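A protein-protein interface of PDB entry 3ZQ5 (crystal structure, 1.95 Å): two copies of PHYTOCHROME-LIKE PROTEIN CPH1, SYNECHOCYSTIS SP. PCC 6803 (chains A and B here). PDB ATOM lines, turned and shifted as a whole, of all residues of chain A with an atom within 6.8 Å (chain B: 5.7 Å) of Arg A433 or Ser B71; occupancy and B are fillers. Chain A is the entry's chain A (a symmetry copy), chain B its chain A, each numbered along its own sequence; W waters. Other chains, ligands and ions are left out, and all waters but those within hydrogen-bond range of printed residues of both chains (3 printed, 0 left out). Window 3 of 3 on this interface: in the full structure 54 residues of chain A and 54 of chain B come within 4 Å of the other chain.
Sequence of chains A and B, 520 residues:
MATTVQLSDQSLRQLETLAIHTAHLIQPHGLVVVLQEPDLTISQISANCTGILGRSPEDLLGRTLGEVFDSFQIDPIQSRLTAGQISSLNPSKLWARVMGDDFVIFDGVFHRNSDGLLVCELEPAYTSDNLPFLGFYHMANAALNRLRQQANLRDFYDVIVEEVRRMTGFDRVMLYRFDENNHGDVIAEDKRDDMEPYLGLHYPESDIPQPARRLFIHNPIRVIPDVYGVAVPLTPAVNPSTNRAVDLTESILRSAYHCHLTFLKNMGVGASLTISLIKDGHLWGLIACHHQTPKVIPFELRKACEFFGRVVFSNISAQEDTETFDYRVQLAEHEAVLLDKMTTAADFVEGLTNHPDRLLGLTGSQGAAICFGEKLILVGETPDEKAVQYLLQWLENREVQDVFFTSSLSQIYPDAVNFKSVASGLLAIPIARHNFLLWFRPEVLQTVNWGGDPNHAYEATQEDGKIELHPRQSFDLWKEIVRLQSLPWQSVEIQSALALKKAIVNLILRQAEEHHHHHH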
ATOM      1  N   GLU A 396     -17.876  28.042  17.148  1.00  0.00           N
ATOM      2  CA  GLU A 396     -19.279  28.428  16.958  1.00  0.00           C
ATOM      3  C   GLU A 396     -19.426  29.722  16.167  1.00  0.00           C
ATOM      4  O   GLU A 396     -20.366  29.870  15.386  1.00  0.00           O
ATOM      5  CB  GLU A 396     -19.997  28.560  18.305  1.00  0.00           C
ATOM      6  CG  GLU A 396     -20.367  27.218  18.912  1.00  0.00           C
ATOM      7  CD  GLU A 396     -21.095  27.333  20.238  1.00  0.00           C
ATOM      8  OE1 GLU A 396     -21.709  28.391  20.501  1.00  0.00           O
ATOM      9  OE2 GLU A 396     -21.059  26.352  21.016  1.00  0.00           O
ATOM     10  N   VAL A 400     -20.403  27.261  10.367  1.00  0.00           N
ATOM     11  CA  VAL A 400     -20.170  25.851  10.675  1.00  0.00           C
ATOM     12  C   VAL A 400     -20.030  25.037   9.386  1.00  0.00           C
ATOM     13  O   VAL A 400     -21.010  24.818   8.673  1.00  0.00           O
ATOM     14  CB  VAL A 400     -21.302  25.283  11.591  1.00  0.00           C
ATOM     15  CG1 VAL A 400     -21.490  23.788  11.387  1.00  0.00           C
ATOM     16  CG2 VAL A 400     -21.007  25.593  13.062  1.00  0.00           C
ATOM     17  N   PRO A 430     -19.193  19.491  13.960  1.00  0.00           N
ATOM     18  CA  PRO A 430     -20.492  19.933  14.490  1.00  0.00           C
ATOM     19  C   PRO A 430     -21.548  18.827  14.416  1.00  0.00           C
ATOM     20  O   PRO A 430     -21.649  18.161  13.392  1.00  0.00           O
ATOM     21  CB  PRO A 430     -20.888  21.095  13.566  1.00  0.00           C
ATOM     22  CG  PRO A 430     -19.697  21.384  12.728  1.00  0.00           C
ATOM     23  CD  PRO A 430     -18.875  20.150  12.681  1.00  0.00           C
ATOM     24  N   ILE A 431     -22.307  18.634  15.494  1.00  0.00           N
ATOM     25  CA  ILE A 431     -23.365  17.624  15.548  1.00  0.00           C
ATOM     26  C   ILE A 431     -24.680  18.299  15.913  1.00  0.00           C
ATOM     27  O   ILE A 431     -24.784  18.911  16.975  1.00  0.00           O
ATOM     28  CB  ILE A 431     -23.087  16.530  16.611  1.00  0.00           C
ATOM     29  CG1 ILE A 431     -21.696  15.922  16.451  1.00  0.00           C
ATOM     30  CG2 ILE A 431     -24.164  15.437  16.551  1.00  0.00           C
ATOM     31  CD1 ILE A 431     -21.327  15.540  15.039  1.00  0.00           C
ATOM     32  N   ALA A 432     -25.681  18.184  15.044  1.00  0.00           N
ATOM     33  CA  ALA A 432     -26.974  18.842  15.267  1.00  0.00           C
ATOM     34  C   ALA A 432     -26.818  20.351  15.467  1.00  0.00           C
ATOM     35  O   ALA A 432     -27.486  20.945  16.316  1.00  0.00           O
ATOM     36  CB  ALA A 432     -27.697  18.218  16.463  1.00  0.00           C
ATOM     37  N   ARG A 433     -25.932  20.954  14.675  1.00  0.00           N
ATOM     38  CA  ARG A 433     -25.567  22.378  14.778  1.00  0.00           C
ATOM     39  C   ARG A 433     -24.834  22.723  16.083  1.00  0.00           C
ATOM     40  O   ARG A 433     -23.617  22.947  16.064  1.00  0.00           O
ATOM     41  CB  ARG A 433     -26.781  23.300  14.538  1.00  0.00           C
ATOM     42  CG  ARG A 433     -26.922  23.774  13.076  1.00  0.00           C
ATOM     43  CD  ARG A 433     -28.376  23.806  12.591  1.00  0.00           C
ATOM     44  NE  ARG A 433     -28.466  23.791  11.128  1.00  0.00           N
ATOM     45  CZ  ARG A 433     -29.585  23.588  10.434  1.00  0.00           C
ATOM     46  NH1 ARG A 433     -30.748  23.382  11.051  1.00  0.00           N
ATOM     47  NH2 ARG A 433     -29.546  23.589   9.105  1.00  0.00           N
ATOM     48  N   HIS A 434     -25.549  22.756  17.209  1.00  0.00           N
ATOM     49  CA  HIS A 434     -25.014  23.401  18.423  1.00  0.00           C
ATOM     50  C   HIS A 434     -23.967  22.573  19.203  1.00  0.00           C
ATOM     51  O   HIS A 434     -23.266  23.122  20.052  1.00  0.00           O
ATOM     52  CB  HIS A 434     -26.150  23.843  19.363  1.00  0.00           C
ATOM     53  CG  HIS A 434     -25.964  25.222  19.918  1.00  0.00           C
ATOM     54  ND1 HIS A 434     -24.739  25.696  20.342  1.00  0.00           N
ATOM     55  CD2 HIS A 434     -26.843  26.237  20.103  1.00  0.00           C
ATOM     56  CE1 HIS A 434     -24.873  26.939  20.768  1.00  0.00           C
ATOM     57  NE2 HIS A 434     -26.140  27.292  20.637  1.00  0.00           N
ATOM     58  N   ASN A 435     -23.859  21.275  18.914  1.00  0.00           N
ATOM     59  CA  ASN A 435     -22.933  20.381  19.638  1.00  0.00           C
ATOM     60  C   ASN A 435     -21.648  20.119  18.854  1.00  0.00           C
ATOM     61  O   ASN A 435     -21.561  20.450  17.672  1.00  0.00           O
ATOM     62  CB  ASN A 435     -23.606  19.039  19.936  1.00  0.00           C
ATOM     63  CG  ASN A 435     -25.026  19.199  20.438  1.00  0.00           C
ATOM     64  OD1 ASN A 435     -25.259  19.789  21.498  1.00  0.00           O
ATOM     65  ND2 ASN A 435     -25.987  18.680  19.670  1.00  0.00           N
ATOM     66  N   PHE A 436     -20.667  19.504  19.510  1.00  0.00           N
ATOM     67  CA  PHE A 436     -19.356  19.220  18.894  1.00  0.00           C
ATOM     68  C   PHE A 436     -18.724  17.963  19.467  1.00  0.00           C
ATOM     69  O   PHE A 436     -18.791  17.713  20.671  1.00  0.00           O
ATOM     70  CB  PHE A 436     -18.374  20.372  19.124  1.00  0.00           C
ATOM     71  CG  PHE A 436     -18.570  21.541  18.210  1.00  0.00           C
ATOM     72  CD1 PHE A 436     -17.967  21.570  16.958  1.00  0.00           C
ATOM     73  CD2 PHE A 436     -19.338  22.632  18.610  1.00  0.00           C
ATOM     74  CE1 PHE A 436     -18.137  22.658  16.120  1.00  0.00           C
ATOM     75  CE2 PHE A 436     -19.514  23.725  17.771  1.00  0.00           C
ATOM     76  CZ  PHE A 436     -18.913  23.737  16.524  1.00  0.00           C
ATOM     77  N   LYS A 501     -20.440  10.952  13.571  1.00  0.00           N
ATOM     78  CA  LYS A 501     -21.418  12.049  13.483  1.00  0.00           C
ATOM     79  C   LYS A 501     -22.751  11.589  12.895  1.00  0.00           C
ATOM     80  O   LYS A 501     -23.814  11.894  13.430  1.00  0.00           O
ATOM     81  CB  LYS A 501     -20.883  13.200  12.634  1.00  0.00           C
ATOM     82  CG  LYS A 501     -21.981  14.127  12.071  1.00  0.00           C
ATOM     83  CD  LYS A 501     -21.410  15.312  11.310  1.00  0.00           C
ATOM     84  CE  LYS A 501     -22.467  16.392  11.095  1.00  0.00           C
ATOM     85  NZ  LYS A 501     -21.886  17.689  10.600  1.00  0.00           N
ATOM     86  N   PHE B  69     -37.517  20.914   3.343  1.00  0.00           N
ATOM     87  CA  PHE B  69     -36.860  19.906   4.195  1.00  0.00           C
ATOM     88  C   PHE B  69     -36.196  20.560   5.387  1.00  0.00           C
ATOM     89  O   PHE B  69     -35.635  21.642   5.263  1.00  0.00           O
ATOM     90  CB  PHE B  69     -35.784  19.154   3.416  1.00  0.00           C
ATOM     91  CG  PHE B  69     -36.296  18.453   2.193  1.00  0.00           C
ATOM     92  CD1 PHE B  69     -36.869  17.191   2.288  1.00  0.00           C
ATOM     93  CD2 PHE B  69     -36.202  19.047   0.950  1.00  0.00           C
ATOM     94  CE1 PHE B  69     -37.348  16.533   1.158  1.00  0.00           C
ATOM     95  CE2 PHE B  69     -36.681  18.393  -0.197  1.00  0.00           C
ATOM     96  CZ  PHE B  69     -37.250  17.133  -0.084  1.00  0.00           C
ATOM     97  N   ASP B  70     -36.252  19.900   6.539  1.00  0.00           N
ATOM     98  CA  ASP B  70     -35.347  20.212   7.643  1.00  0.00           C
ATOM     99  C   ASP B  70     -34.054  19.398   7.512  1.00  0.00           C
ATOM    100  O   ASP B  70     -34.049  18.298   6.947  1.00  0.00           O
ATOM    101  CB  ASP B  70     -36.010  19.934   8.996  1.00  0.00           C
ATOM    102  CG  ASP B  70     -37.146  20.895   9.304  1.00  0.00           C
ATOM    103  OD1 ASP B  70     -37.101  22.059   8.842  1.00  0.00           O
ATOM    104  OD2 ASP B  70     -38.087  20.487  10.018  1.00  0.00           O
ATOM    105  N   SER B  71     -32.961  19.963   8.025  1.00  0.00           N
ATOM    106  CA  SER B  71     -31.676  19.283   8.072  1.00  0.00           C
ATOM    107  C   SER B  71     -30.805  19.901   9.155  1.00  0.00           C
ATOM    108  O   SER B  71     -31.083  21.007   9.626  1.00  0.00           O
ATOM    109  CB  SER B  71     -30.958  19.389   6.728  1.00  0.00           C
ATOM    110  OG  SER B  71     -30.190  20.579   6.662  1.00  0.00           O
ATOM    111  N   PHE B  72     -29.751  19.186   9.541  1.00  0.00           N
ATOM    112  CA  PHE B  72     -28.758  19.713  10.480  1.00  0.00           C
ATOM    113  C   PHE B  72     -27.594  20.382   9.760  1.00  0.00           C
ATOM    114  O   PHE B  72     -27.026  21.344  10.267  1.00  0.00           O
ATOM    115  CB  PHE B  72     -28.212  18.604  11.389  1.00  0.00           C
ATOM    116  CG  PHE B  72     -29.214  18.068  12.372  1.00  0.00           C
ATOM    117  CD1 PHE B  72     -29.822  18.907  13.292  1.00  0.00           C
ATOM    118  CD2 PHE B  72     -29.534  16.720  12.393  1.00  0.00           C
ATOM    119  CE1 PHE B  72     -30.736  18.416  14.209  1.00  0.00           C
ATOM    120  CE2 PHE B  72     -30.451  16.221  13.311  1.00  0.00           C
ATOM    121  CZ  PHE B  72     -31.051  17.072  14.217  1.00  0.00           C
ATOM    122  N   GLN B  73     -27.262  19.882   8.572  1.00  0.00           N
ATOM    123  CA  GLN B  73     -25.928  20.131   8.014  1.00  0.00           C
ATOM    124  C   GLN B  73     -25.940  21.045   6.783  1.00  0.00           C
ATOM    125  O   GLN B  73     -24.877  21.524   6.368  1.00  0.00           O
ATOM    126  CB  GLN B  73     -25.129  18.825   7.762  1.00  0.00           C
ATOM    127  CG  GLN B  73     -25.913  17.562   7.367  1.00  0.00           C
ATOM    128  CD  GLN B  73     -25.895  16.467   8.446  1.00  0.00           C
ATOM    129  OE1 GLN B  73     -25.737  16.749   9.634  1.00  0.00           O
ATOM    130  NE2 GLN B  73     -26.060  15.211   8.025  1.00  0.00           N
ATOM    131  N   ILE B  74     -27.124  21.334   6.231  1.00  0.00           N
ATOM    132  CA  ILE B  74     -27.239  22.254   5.091  1.00  0.00           C
ATOM    133  C   ILE B  74     -27.612  23.660   5.564  1.00  0.00           C
ATOM    134  O   ILE B  74     -28.784  23.959   5.797  1.00  0.00           O
ATOM    135  CB  ILE B  74     -28.275  21.764   4.043  1.00  0.00           C
ATOM    136  CG1 ILE B  74     -27.839  20.427   3.424  1.00  0.00           C
ATOM    137  CG2 ILE B  74     -28.464  22.810   2.943  1.00  0.00           C
ATOM    138  CD1 ILE B  74     -28.764  19.262   3.748  1.00  0.00           C
ATOM    139  N   ASP B  75     -26.597  24.512   5.702  1.00  0.00           N
ATOM    140  CA  ASP B  75     -26.782  25.901   6.119  1.00  0.00           C
ATOM    141  C   ASP B  75     -26.959  26.787   4.884  1.00  0.00           C
ATOM    142  O   ASP B  75     -26.560  26.402   3.780  1.00  0.00           O
ATOM    143  CB  ASP B  75     -25.575  26.397   6.930  1.00  0.00           C
ATOM    144  CG  ASP B  75     -25.093  25.383   7.964  1.00  0.00           C
ATOM    145  OD1 ASP B  75     -24.576  24.316   7.561  1.00  0.00           O
ATOM    146  OD2 ASP B  75     -25.218  25.660   9.177  1.00  0.00           O
ATOM    147  N   LYS B  93     -28.639  13.660   6.393  1.00  0.00           N
ATOM    148  CA  LYS B  93     -30.060  13.502   6.707  1.00  0.00           C
ATOM    149  C   LYS B  93     -30.822  14.763   6.316  1.00  0.00           C
ATOM    150  O   LYS B  93     -30.399  15.873   6.637  1.00  0.00           O
ATOM    151  CB  LYS B  93     -30.285  13.187   8.190  1.00  0.00           C
ATOM    152  CG  LYS B  93     -29.937  11.745   8.572  1.00  0.00           C
ATOM    153  CD  LYS B  93     -30.985  10.758   8.048  1.00  0.00           C
ATOM    154  CE  LYS B  93     -30.722   9.317   8.493  1.00  0.00           C
ATOM    155  NZ  LYS B  93     -29.332   8.842   8.199  1.00  0.00           N
ATOM    156  N   LEU B  94     -31.915  14.567   5.585  1.00  0.00           N
ATOM    157  CA  LEU B  94     -32.938  15.577   5.374  1.00  0.00           C
ATOM    158  C   LEU B  94     -34.281  14.935   5.688  1.00  0.00           C
ATOM    159  O   LEU B  94     -34.501  13.758   5.363  1.00  0.00           O
ATOM    160  CB  LEU B  94     -32.948  16.030   3.910  1.00  0.00           C
ATOM    161  CG  LEU B  94     -31.815  16.951   3.472  1.00  0.00           C
ATOM    162  CD1 LEU B  94     -30.597  16.135   3.050  1.00  0.00           C
ATOM    163  CD2 LEU B  94     -32.271  17.852   2.335  1.00  0.00           C
ATOM    164  N   TRP B  95     -35.196  15.690   6.293  1.00  0.00           N
ATOM    165  CA  TRP B  95     -36.525  15.153   6.556  1.00  0.00           C
ATOM    166  C   TRP B  95     -37.599  16.202   6.360  1.00  0.00           C
ATOM    167  O   TRP B  95     -37.351  17.398   6.502  1.00  0.00           O
ATOM    168  CB  TRP B  95     -36.612  14.524   7.961  1.00  0.00           C
ATOM    169  CG  TRP B  95     -36.338  15.486   9.075  1.00  0.00           C
ATOM    170  CD1 TRP B  95     -37.262  16.133   9.845  1.00  0.00           C
ATOM    171  CD2 TRP B  95     -35.053  15.926   9.535  1.00  0.00           C
ATOM    172  NE1 TRP B  95     -36.632  16.948  10.758  1.00  0.00           N
ATOM    173  CE2 TRP B  95     -35.276  16.843  10.586  1.00  0.00           C
ATOM    174  CE3 TRP B  95     -33.735  15.640   9.155  1.00  0.00           C
ATOM    175  CZ2 TRP B  95     -34.234  17.467  11.266  1.00  0.00           C
ATOM    176  CZ3 TRP B  95     -32.704  16.262   9.825  1.00  0.00           C
ATOM    177  CH2 TRP B  95     -32.958  17.166  10.872  1.00  0.00           C
HETATM  178  O   HOH W   1     -32.726  21.921  12.556  1.00  0.00           O
HETATM  179  O   HOH W   2     -24.345  20.475  12.206  1.00  0.00           O
HETATM  180  O   HOH W   3     -33.443  22.720   9.110  1.00  0.00           O
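The backbone carbonyl oxygen (O) of Ser B71 lies within hydrogen-bond range of the guanidinium group (NH1) of Arg A433, 2.8 Å away.
The guanidinium group (NE) of Arg A433 lies within hydrogen-bond range of the backbone carbonyl oxygen (O) of Phe B72 (3.0 Å).
NH2 of Arg A433 is in hydrogen-bond range of O of Ile B74.
The side-chain hydroxyl of Ser B71 is in hydrogen-bond range of the backbone NH of Ile B74, 3.2 Å away.
The side-chain amide nitrogen (NE2) of Gln B73 lies close to the backbone NH (N) of Lys B93 (3.4 Å).
O of Pro A430 sits at hydrogen-bond distance from NZ of Lys A501 (2.8 Å).
Among the printed residues, pairs that only touch across the chains: Ala A432 with Phe B72 (3.5 Å), Lys A501 with Gln B73 (3.6 Å) and Val A400 with Asp B75 (3.8 Å).
Printed residues of chain B within 4 Å of Val A400: Asp B75 (3.8 Å).
Printed residues of chain B within 4 Å of Ala A432: Phe B72.
Arg A433 touches just these residues of chain B: Ser B71, Phe B72 and Ile B74.
Printed residues of chain A within 4 Å of Ser B71: Arg A433.
Printed residues of chain A within 4 Å of Phe B72: Ala A432 (3.5 Å) and Arg A433 (3.0 Å).
Of the printed residues of chain A, Gln B73 touches Lys A501.
Of the printed residues of chain A, Ile B74 touches Arg A433.
Hydrophobic or aromatic side chains of chain B that line the printed part of chain A: Phe B72.
Printed residues of chain A that touch a printed residue of chain B: Val A400, Ala A432, Arg A433 and Lys A501.
Hydrophobic or aromatic side chains of chain A within 4 Å of the printed part of chain B: Ala A432.
Among the printed residues, 6 pairs touch across the chains.
No position is printed for both chains.
Water W1 lies within hydrogen-bond range of the guanidinium group of Arg A433 (2.9 Å) and the backbone carbonyl oxygen of Ser B71 (3.5 Å).
Water W3 lies within hydrogen-bond range of O of Ser B71 (3.0 Å) and NH1 of Arg A433 (3.4 Å).
Water W2 bridges the backbone NH of Arg A433 (3.0 Å) and the backbone carbonyl oxygen of Phe B72 (3.4 Å).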
